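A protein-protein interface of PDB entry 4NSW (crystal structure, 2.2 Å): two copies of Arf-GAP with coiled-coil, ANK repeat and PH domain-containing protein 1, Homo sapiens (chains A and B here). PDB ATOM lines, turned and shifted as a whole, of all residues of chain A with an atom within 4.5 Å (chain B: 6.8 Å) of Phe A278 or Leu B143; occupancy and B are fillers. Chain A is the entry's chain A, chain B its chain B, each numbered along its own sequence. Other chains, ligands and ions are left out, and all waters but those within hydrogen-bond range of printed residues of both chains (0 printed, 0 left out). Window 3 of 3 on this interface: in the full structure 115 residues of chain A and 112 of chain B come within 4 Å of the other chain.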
ATOM      1  N   GLU A 259      28.255 -36.042  14.908  1.00  0.00           N
ATOM      2  CA  GLU A 259      29.102 -34.849  14.999  1.00  0.00           C
ATOM      3  C   GLU A 259      30.567 -35.285  15.063  1.00  0.00           C
ATOM      4  O   GLU A 259      30.862 -36.380  15.557  1.00  0.00           O
ATOM      5  CB  GLU A 259      28.780 -34.027  16.256  1.00  0.00           C
ATOM      6  CG  GLU A 259      27.542 -33.137  16.191  1.00  0.00           C
ATOM      7  CD  GLU A 259      27.624 -32.049  15.119  1.00  0.00           C
ATOM      8  OE1 GLU A 259      28.363 -31.048  15.302  1.00  0.00           O
ATOM      9  OE2 GLU A 259      26.925 -32.197  14.098  1.00  0.00           O
ATOM     10  N   LEU A 277      32.866 -25.522  19.929  1.00  0.00           N
ATOM     11  CA  LEU A 277      31.876 -25.411  21.001  1.00  0.00           C
ATOM     12  C   LEU A 277      31.146 -24.070  20.840  1.00  0.00           C
ATOM     13  O   LEU A 277      31.718 -23.085  20.347  1.00  0.00           O
ATOM     14  CB  LEU A 277      32.522 -25.504  22.388  1.00  0.00           C
ATOM     15  CG  LEU A 277      33.210 -26.786  22.923  1.00  0.00           C
ATOM     16  CD1 LEU A 277      33.894 -26.548  24.248  1.00  0.00           C
ATOM     17  CD2 LEU A 277      32.215 -27.933  23.062  1.00  0.00           C
ATOM     18  N   PHE A 278      29.869 -24.047  21.221  1.00  0.00           N
ATOM     19  CA  PHE A 278      29.146 -22.798  21.369  1.00  0.00           C
ATOM     20  C   PHE A 278      29.558 -22.188  22.714  1.00  0.00           C
ATOM     21  O   PHE A 278      29.720 -22.893  23.726  1.00  0.00           O
ATOM     22  CB  PHE A 278      27.628 -23.021  21.347  1.00  0.00           C
ATOM     23  CG  PHE A 278      27.049 -23.268  19.974  1.00  0.00           C
ATOM     24  CD1 PHE A 278      26.631 -22.205  19.177  1.00  0.00           C
ATOM     25  CD2 PHE A 278      26.897 -24.565  19.485  1.00  0.00           C
ATOM     26  CE1 PHE A 278      26.077 -22.427  17.900  1.00  0.00           C
ATOM     27  CE2 PHE A 278      26.352 -24.799  18.213  1.00  0.00           C
ATOM     28  CZ  PHE A 278      25.933 -23.723  17.426  1.00  0.00           C
ATOM     29  N   LYS A 279      29.738 -20.880  22.727  1.00  0.00           N
ATOM     30  CA  LYS A 279      30.027 -20.211  23.960  1.00  0.00           C
ATOM     31  C   LYS A 279      29.166 -18.969  24.122  1.00  0.00           C
ATOM     32  O   LYS A 279      29.101 -18.116  23.229  1.00  0.00           O
ATOM     33  CB  LYS A 279      31.521 -19.894  24.086  1.00  0.00           C
ATOM     34  CG  LYS A 279      32.085 -19.063  22.981  1.00  0.00           C
ATOM     35  CD  LYS A 279      32.949 -17.952  23.533  1.00  0.00           C
ATOM     36  CE  LYS A 279      33.229 -16.915  22.445  1.00  0.00           C
ATOM     37  NZ  LYS A 279      31.995 -16.426  21.764  1.00  0.00           N
ATOM     38  N   ARG A 280      28.479 -18.903  25.261  1.00  0.00           N
ATOM     39  CA  ARG A 280      27.827 -17.679  25.710  1.00  0.00           C
ATOM     40  C   ARG A 280      28.950 -16.701  26.023  1.00  0.00           C
ATOM     41  O   ARG A 280      29.946 -17.075  26.644  1.00  0.00           O
ATOM     42  CB  ARG A 280      26.983 -17.951  26.960  1.00  0.00           C
ATOM     43  CG  ARG A 280      26.294 -16.719  27.529  1.00  0.00           C
ATOM     44  CD  ARG A 280      25.714 -16.959  28.921  1.00  0.00           C
ATOM     45  NE  ARG A 280      24.464 -17.725  28.912  1.00  0.00           N
ATOM     46  CZ  ARG A 280      23.259 -17.227  28.630  1.00  0.00           C
ATOM     47  NH1 ARG A 280      23.109 -15.944  28.312  1.00  0.00           N
ATOM     48  NH2 ARG A 280      22.195 -18.021  28.654  1.00  0.00           N
ATOM     49  N   TRP A 288      25.106 -16.849  22.131  1.00  0.00           N
ATOM     50  CA  TRP A 288      25.652 -18.169  21.868  1.00  0.00           C
ATOM     51  C   TRP A 288      26.388 -18.100  20.531  1.00  0.00           C
ATOM     52  O   TRP A 288      25.773 -18.025  19.461  1.00  0.00           O
ATOM     53  CB  TRP A 288      24.547 -19.240  21.881  1.00  0.00           C
ATOM     54  CG  TRP A 288      23.995 -19.477  23.259  1.00  0.00           C
ATOM     55  CD1 TRP A 288      22.797 -19.048  23.749  1.00  0.00           C
ATOM     56  CD2 TRP A 288      24.648 -20.164  24.338  1.00  0.00           C
ATOM     57  NE1 TRP A 288      22.655 -19.434  25.064  1.00  0.00           N
ATOM     58  CE2 TRP A 288      23.773 -20.126  25.446  1.00  0.00           C
ATOM     59  CE3 TRP A 288      25.879 -20.820  24.468  1.00  0.00           C
ATOM     60  CZ2 TRP A 288      24.091 -20.712  26.667  1.00  0.00           C
ATOM     61  CZ3 TRP A 288      26.195 -21.403  25.682  1.00  0.00           C
ATOM     62  CH2 TRP A 288      25.305 -21.347  26.765  1.00  0.00           C
ATOM     63  N   SER A 289      27.713 -18.075  20.628  1.00  0.00           N
ATOM     64  CA  SER A 289      28.604 -17.969  19.485  1.00  0.00           C
ATOM     65  C   SER A 289      29.477 -19.221  19.394  1.00  0.00           C
ATOM     66  O   SER A 289      30.106 -19.622  20.367  1.00  0.00           O
ATOM     67  CB  SER A 289      29.483 -16.730  19.649  1.00  0.00           C
ATOM     68  OG  SER A 289      30.091 -16.349  18.432  1.00  0.00           O
ATOM     69  N   ARG A 290      29.507 -19.827  18.215  1.00  0.00           N
ATOM     70  CA  ARG A 290      30.247 -21.052  17.986  1.00  0.00           C
ATOM     71  C   ARG A 290      31.701 -20.715  17.647  1.00  0.00           C
ATOM     72  O   ARG A 290      31.971 -19.987  16.684  1.00  0.00           O
ATOM     73  CB  ARG A 290      29.578 -21.857  16.882  1.00  0.00           C
ATOM     74  CG  ARG A 290      30.224 -23.197  16.561  1.00  0.00           C
ATOM     75  CD  ARG A 290      29.224 -24.061  15.835  1.00  0.00           C
ATOM     76  NE  ARG A 290      29.772 -25.292  15.271  1.00  0.00           N
ATOM     77  CZ  ARG A 290      29.656 -26.501  15.820  1.00  0.00           C
ATOM     78  NH1 ARG A 290      29.045 -26.657  16.994  1.00  0.00           N
ATOM     79  NH2 ARG A 290      30.165 -27.561  15.198  1.00  0.00           N
ATOM     80  N   LEU A 344      30.669 -20.072  30.178  1.00  0.00           N
ATOM     81  CA  LEU A 344      29.638 -21.063  29.881  1.00  0.00           C
ATOM     82  C   LEU A 344      29.897 -21.610  28.479  1.00  0.00           C
ATOM     83  O   LEU A 344      30.180 -20.854  27.561  1.00  0.00           O
ATOM     84  CB  LEU A 344      28.241 -20.448  29.960  1.00  0.00           C
ATOM     85  CG  LEU A 344      27.173 -21.254  30.715  1.00  0.00           C
ATOM     86  CD1 LEU A 344      25.963 -20.353  31.142  1.00  0.00           C
ATOM     87  CD2 LEU A 344      26.718 -22.522  29.978  1.00  0.00           C
ATOM     88  N   LEU A 345      29.832 -22.929  28.346  1.00  0.00           N
ATOM     89  CA  LEU A 345      30.194 -23.618  27.112  1.00  0.00           C
ATOM     90  C   LEU A 345      29.090 -24.590  26.778  1.00  0.00           C
ATOM     91  O   LEU A 345      28.425 -25.122  27.669  1.00  0.00           O
ATOM     92  CB  LEU A 345      31.501 -24.383  27.264  1.00  0.00           C
ATOM     93  CG  LEU A 345      32.787 -23.646  27.632  1.00  0.00           C
ATOM     94  CD1 LEU A 345      33.973 -24.612  27.605  1.00  0.00           C
ATOM     95  CD2 LEU A 345      33.032 -22.491  26.707  1.00  0.00           C
ATOM     96  N   GLN A 346      28.876 -24.820  25.495  1.00  0.00           N
ATOM     97  CA  GLN A 346      27.799 -25.698  25.115  1.00  0.00           C
ATOM     98  C   GLN A 346      28.251 -26.608  24.002  1.00  0.00           C
ATOM     99  O   GLN A 346      28.748 -26.152  22.982  1.00  0.00           O
ATOM    100  CB  GLN A 346      26.579 -24.884  24.708  1.00  0.00           C
ATOM    101  CG  GLN A 346      25.421 -25.727  24.299  1.00  0.00           C
ATOM    102  CD  GLN A 346      24.370 -24.937  23.572  1.00  0.00           C
ATOM    103  OE1 GLN A 346      23.243 -25.396  23.438  1.00  0.00           O
ATOM    104  NE2 GLN A 346      24.719 -23.733  23.116  1.00  0.00           N
ATOM    105  N   ASP A 348      27.330 -29.925  21.316  1.00  0.00           N
ATOM    106  CA  ASP A 348      26.230 -30.162  20.380  1.00  0.00           C
ATOM    107  C   ASP A 348      25.385 -31.385  20.687  1.00  0.00           C
ATOM    108  O   ASP A 348      24.284 -31.511  20.169  1.00  0.00           O
ATOM    109  CB  ASP A 348      26.769 -30.258  18.953  1.00  0.00           C
ATOM    110  CG  ASP A 348      27.379 -28.971  18.496  1.00  0.00           C
ATOM    111  OD1 ASP A 348      26.648 -27.966  18.416  1.00  0.00           O
ATOM    112  OD2 ASP A 348      28.597 -28.952  18.235  1.00  0.00           O
ATOM    113  N   ASP B  18      36.171 -30.729  10.202  1.00  0.00           N
ATOM    114  CA  ASP B  18      35.493 -29.445   9.914  1.00  0.00           C
ATOM    115  C   ASP B  18      36.149 -28.247  10.631  1.00  0.00           C
ATOM    116  O   ASP B  18      35.476 -27.452  11.291  1.00  0.00           O
ATOM    117  CB  ASP B  18      33.997 -29.526  10.255  1.00  0.00           C
ATOM    118  CG  ASP B  18      33.190 -28.354   9.684  1.00  0.00           C
ATOM    119  OD1 ASP B  18      33.586 -27.789   8.653  1.00  0.00           O
ATOM    120  OD2 ASP B  18      32.147 -28.003  10.272  1.00  0.00           O
ATOM    121  N   SER B 138      23.131 -24.728   5.389  1.00  0.00           N
ATOM    122  CA  SER B 138      22.096 -25.492   6.074  1.00  0.00           C
ATOM    123  C   SER B 138      22.606 -26.223   7.320  1.00  0.00           C
ATOM    124  O   SER B 138      21.836 -26.489   8.231  1.00  0.00           O
ATOM    125  CB  SER B 138      21.376 -26.430   5.106  1.00  0.00           C
ATOM    126  OG  SER B 138      21.884 -27.744   5.168  1.00  0.00           O
ATOM    127  N   LEU B 139      23.897 -26.552   7.363  1.00  0.00           N
ATOM    128  CA  LEU B 139      24.486 -27.127   8.568  1.00  0.00           C
ATOM    129  C   LEU B 139      24.585 -26.074   9.672  1.00  0.00           C
ATOM    130  O   LEU B 139      24.259 -26.370  10.806  1.00  0.00           O
ATOM    131  CB  LEU B 139      25.852 -27.796   8.313  1.00  0.00           C
ATOM    132  CG  LEU B 139      26.639 -28.364   9.522  1.00  0.00           C
ATOM    133  CD1 LEU B 139      25.873 -29.449  10.276  1.00  0.00           C
ATOM    134  CD2 LEU B 139      28.043 -28.856   9.153  1.00  0.00           C
ATOM    135  N   GLU B 140      25.014 -24.860   9.326  1.00  0.00           N
ATOM    136  CA  GLU B 140      25.137 -23.768  10.291  1.00  0.00           C
ATOM    137  C   GLU B 140      23.782 -23.378  10.874  1.00  0.00           C
ATOM    138  O   GLU B 140      23.708 -22.849  11.992  1.00  0.00           O
ATOM    139  CB  GLU B 140      25.845 -22.559   9.675  1.00  0.00           C
ATOM    140  CG  GLU B 140      26.524 -21.644  10.695  1.00  0.00           C
ATOM    141  CD  GLU B 140      25.828 -20.294  10.851  1.00  0.00           C
ATOM    142  OE1 GLU B 140      25.231 -20.011  11.938  1.00  0.00           O
ATOM    143  OE2 GLU B 140      25.882 -19.516   9.878  1.00  0.00           O
ATOM    144  N   ALA B 141      22.712 -23.662  10.129  1.00  0.00           N
ATOM    145  CA  ALA B 141      21.351 -23.485  10.626  1.00  0.00           C
ATOM    146  C   ALA B 141      20.986 -24.593  11.609  1.00  0.00           C
ATOM    147  O   ALA B 141      20.344 -24.344  12.643  1.00  0.00           O
ATOM    148  CB  ALA B 141      20.359 -23.456   9.471  1.00  0.00           C
ATOM    149  N   ALA B 142      21.389 -25.815  11.277  1.00  0.00           N
ATOM    150  CA  ALA B 142      21.024 -26.987  12.058  1.00  0.00           C
ATOM    151  C   ALA B 142      21.736 -27.020  13.419  1.00  0.00           C
ATOM    152  O   ALA B 142      21.140 -27.385  14.410  1.00  0.00           O
ATOM    153  CB  ALA B 142      21.302 -28.244  11.272  1.00  0.00           C
ATOM    154  N   LEU B 143      23.006 -26.616  13.439  1.00  0.00           N
ATOM    155  CA  LEU B 143      23.792 -26.486  14.664  1.00  0.00           C
ATOM    156  C   LEU B 143      23.213 -25.488  15.670  1.00  0.00           C
ATOM    157  O   LEU B 143      23.136 -25.801  16.840  1.00  0.00           O
ATOM    158  CB  LEU B 143      25.241 -26.094  14.324  1.00  0.00           C
ATOM    159  CG  LEU B 143      26.143 -27.188  13.745  1.00  0.00           C
ATOM    160  CD1 LEU B 143      27.387 -26.585  13.077  1.00  0.00           C
ATOM    161  CD2 LEU B 143      26.514 -28.223  14.810  1.00  0.00           C
ATOM    162  N   THR B 144      22.837 -24.291  15.213  1.00  0.00           N
ATOM    163  CA  THR B 144      22.294 -23.227  16.089  1.00  0.00           C
ATOM    164  C   THR B 144      20.900 -23.567  16.596  1.00  0.00           C
ATOM    165  O   THR B 144      20.589 -23.360  17.773  1.00  0.00           O
ATOM    166  CB  THR B 144      22.193 -21.872  15.364  1.00  0.00           C
ATOM    167  OG1 THR B 144      21.520 -22.060  14.112  1.00  0.00           O
ATOM    168  CG2 THR B 144      23.570 -21.289  15.095  1.00  0.00           C
ATOM    169  N   HIS B 145      20.063 -24.078  15.695  1.00  0.00           N
ATOM    170  CA  HIS B 145      18.735 -24.534  16.052  1.00  0.00           C
ATOM    171  C   HIS B 145      18.805 -25.605  17.148  1.00  0.00           C
ATOM    172  O   HIS B 145      18.112 -25.510  18.164  1.00  0.00           O
ATOM    173  CB  HIS B 145      17.964 -25.044  14.823  1.00  0.00           C
ATOM    174  CG  HIS B 145      16.643 -25.664  15.168  1.00  0.00           C
ATOM    175  ND1 HIS B 145      15.654 -24.975  15.839  1.00  0.00           N
ATOM    176  CD2 HIS B 145      16.167 -26.918  14.979  1.00  0.00           C
ATOM    177  CE1 HIS B 145      14.624 -25.777  16.045  1.00  0.00           C
ATOM    178  NE2 HIS B 145      14.909 -26.961  15.531  1.00  0.00           N
ATOM    179  N   ASN B 146      19.657 -26.606  16.940  1.00  0.00           N
ATOM    180  CA  ASN B 146      19.875 -27.685  17.902  1.00  0.00           C
ATOM    181  C   ASN B 146      20.487 -27.179  19.209  1.00  0.00           C
ATOM    182  O   ASN B 146      20.287 -27.785  20.260  1.00  0.00           O
ATOM    183  CB  ASN B 146      20.733 -28.774  17.251  1.00  0.00           C
ATOM    184  CG  ASN B 146      21.144 -29.851  18.210  1.00  0.00           C
ATOM    185  OD1 ASN B 146      22.080 -29.678  18.983  1.00  0.00           O
ATOM    186  ND2 ASN B 146      20.473 -30.990  18.141  1.00  0.00           N
ATOM    187  N   ALA B 147      21.190 -26.049  19.146  1.00  0.00           N
ATOM    188  CA  ALA B 147      21.763 -25.402  20.328  1.00  0.00           C
ATOM    189  C   ALA B 147      20.746 -24.579  21.113  1.00  0.00           C
ATOM    190  O   ALA B 147      20.729 -24.615  22.343  1.00  0.00           O
ATOM    191  CB  ALA B 147      22.939 -24.526  19.941  1.00  0.00           C
ATOM    192  N   GLU B 148      19.913 -23.823  20.401  1.00  0.00           N
ATOM    193  CA  GLU B 148      19.011 -22.858  21.037  1.00  0.00           C
ATOM    194  C   GLU B 148      17.702 -23.458  21.542  1.00  0.00           C
ATOM    195  O   GLU B 148      16.928 -22.774  22.220  1.00  0.00           O
ATOM    196  CB  GLU B 148      18.745 -21.671  20.108  1.00  0.00           C
ATOM    197  CG  GLU B 148      19.837 -20.612  20.162  1.00  0.00           C
ATOM    198  CD  GLU B 148      19.670 -19.521  19.122  1.00  0.00           C
ATOM    199  OE1 GLU B 148      19.285 -19.829  17.973  1.00  0.00           O
ATOM    200  OE2 GLU B 148      19.938 -18.347  19.461  1.00  0.00           O
ATOM    201  N   LEU B 164      19.869 -32.176  12.557  1.00  0.00           N
ATOM    202  CA  LEU B 164      21.299 -31.895  12.625  1.00  0.00           C
ATOM    203  C   LEU B 164      22.051 -33.059  12.017  1.00  0.00           C
ATOM    204  O   LEU B 164      23.015 -32.863  11.296  1.00  0.00           O
ATOM    205  CB  LEU B 164      21.737 -31.693  14.078  1.00  0.00           C
ATOM    206  CG  LEU B 164      23.226 -31.694  14.490  1.00  0.00           C
ATOM    207  CD1 LEU B 164      23.426 -30.926  15.791  1.00  0.00           C
ATOM    208  CD2 LEU B 164      23.828 -33.097  14.622  1.00  0.00           C
ATOM    209  N   ALA B 167      21.871 -32.839   8.214  1.00  0.00           N
ATOM    210  CA  ALA B 167      22.684 -31.718   7.729  1.00  0.00           C
ATOM    211  C   ALA B 167      24.176 -32.021   7.856  1.00  0.00           C
ATOM    212  O   ALA B 167      24.949 -31.631   7.003  1.00  0.00           O
ATOM    213  CB  ALA B 167      22.335 -30.421   8.434  1.00  0.00           C
ATOM    214  N   ARG B 168      24.568 -32.741   8.905  1.00  0.00           N
ATOM    215  CA  ARG B 168      25.965 -33.160   9.057  1.00  0.00           C
ATOM    216  C   ARG B 168      26.376 -34.211   8.013  1.00  0.00           C
ATOM    217  O   ARG B 168      27.424 -34.100   7.382  1.00  0.00           O
ATOM    218  CB  ARG B 168      26.246 -33.660  10.488  1.00  0.00           C
ATOM    219  CG  ARG B 168      27.598 -34.360  10.672  1.00  0.00           C
ATOM    220  CD  ARG B 168      28.766 -33.393  10.487  1.00  0.00           C
ATOM    221  NE  ARG B 168      28.697 -32.328  11.488  1.00  0.00           N
ATOM    222  CZ  ARG B 168      29.492 -31.264  11.516  1.00  0.00           C
ATOM    223  NH1 ARG B 168      30.435 -31.111  10.590  1.00  0.00           N
ATOM    224  NH2 ARG B 168      29.341 -30.362  12.474  1.00  0.00           N
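NH2 of Arg B168 lies within salt-bridge range of OE1 of Glu A259, 3.1 Å away. The side-chain amide oxygen (OE1) of Gln A346 sits close to the backbone carbonyl oxygen (O) of Ala B147 (2.9 Å). O of Asp A348 sits close to OD1 of Asn B146 (3.1 Å).
NH1 of Arg A290 lies within salt-bridge range of OD2 of Asp A348 (2.6 Å). The backbone carbonyl oxygen (O) of Phe A278 sits at hydrogen-bond distance from the backbone NH (N) of Gln A346, 2.7 Å away. O of Ala B141 is in hydrogen-bond range of OG1 of Thr B144 (3.0 Å). The guanidinium group of Arg A290 lies within salt-bridge range of the side-chain carboxylate of Glu A259. OD2 of Asp B18 lies within salt-bridge range of NH1 of Arg B168 (3.6 Å). The side-chain hydroxyl (OG1) of Thr B144 lies within hydrogen-bond range of the backbone carbonyl oxygen (O) of Glu B140 (3.1 Å).
Among the printed residues, merely in contact across the chains: Glu A259 with Leu B164, Glu A259 with Leu B143, Arg A290 with Leu B143, Phe A278 with Leu B143, Asp A348 with Leu B143, Phe A278 with Ala B147, Phe A278 with Thr B144 and Arg A290 with Arg B168.
Printed residues of chain A within 4 Å of Leu B143: Glu A259, Phe A278, Arg A290 and Asp A348. Of the printed residues of chain B, Arg A290 touches Leu B143 and Arg B168. Of the printed residues of chain A, Leu B164 touches Glu A259. Of the printed residues of chain A, Ala B147 touches Phe A278 and Gln A346. Of the printed residues of chain B, Asp A348 touches Leu B143 and Asn B146. Ala B167 touches none of the printed residues of chain A. The nearest printed residue of chain A that does not touch Arg B168 is Asp A348 (6.0 Å).
Of the 12 printed residues of chain A, 5 touch a printed residue of chain B. Hydrophobic or aromatic side chains of chain A within 4 Å of the printed part of chain B: Phe A278. Printed residues of chain B that touch a printed residue of chain A: Leu B143, Thr B144, Asn B146, Ala B147, Leu B164 and Arg B168. Hydrophobic or aromatic side chains of chain B within 4 Å of the printed part of chain A: Leu B143, Ala B147 and Leu B164. Among the printed residues, 11 pairs touch across the chains. Among the printed residues, Asp or Glu carboxylates within 4 Å of a Lys or Arg side-chain nitrogen of the other chain: Glu A259 with Arg B168.
No position is printed for both chains.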
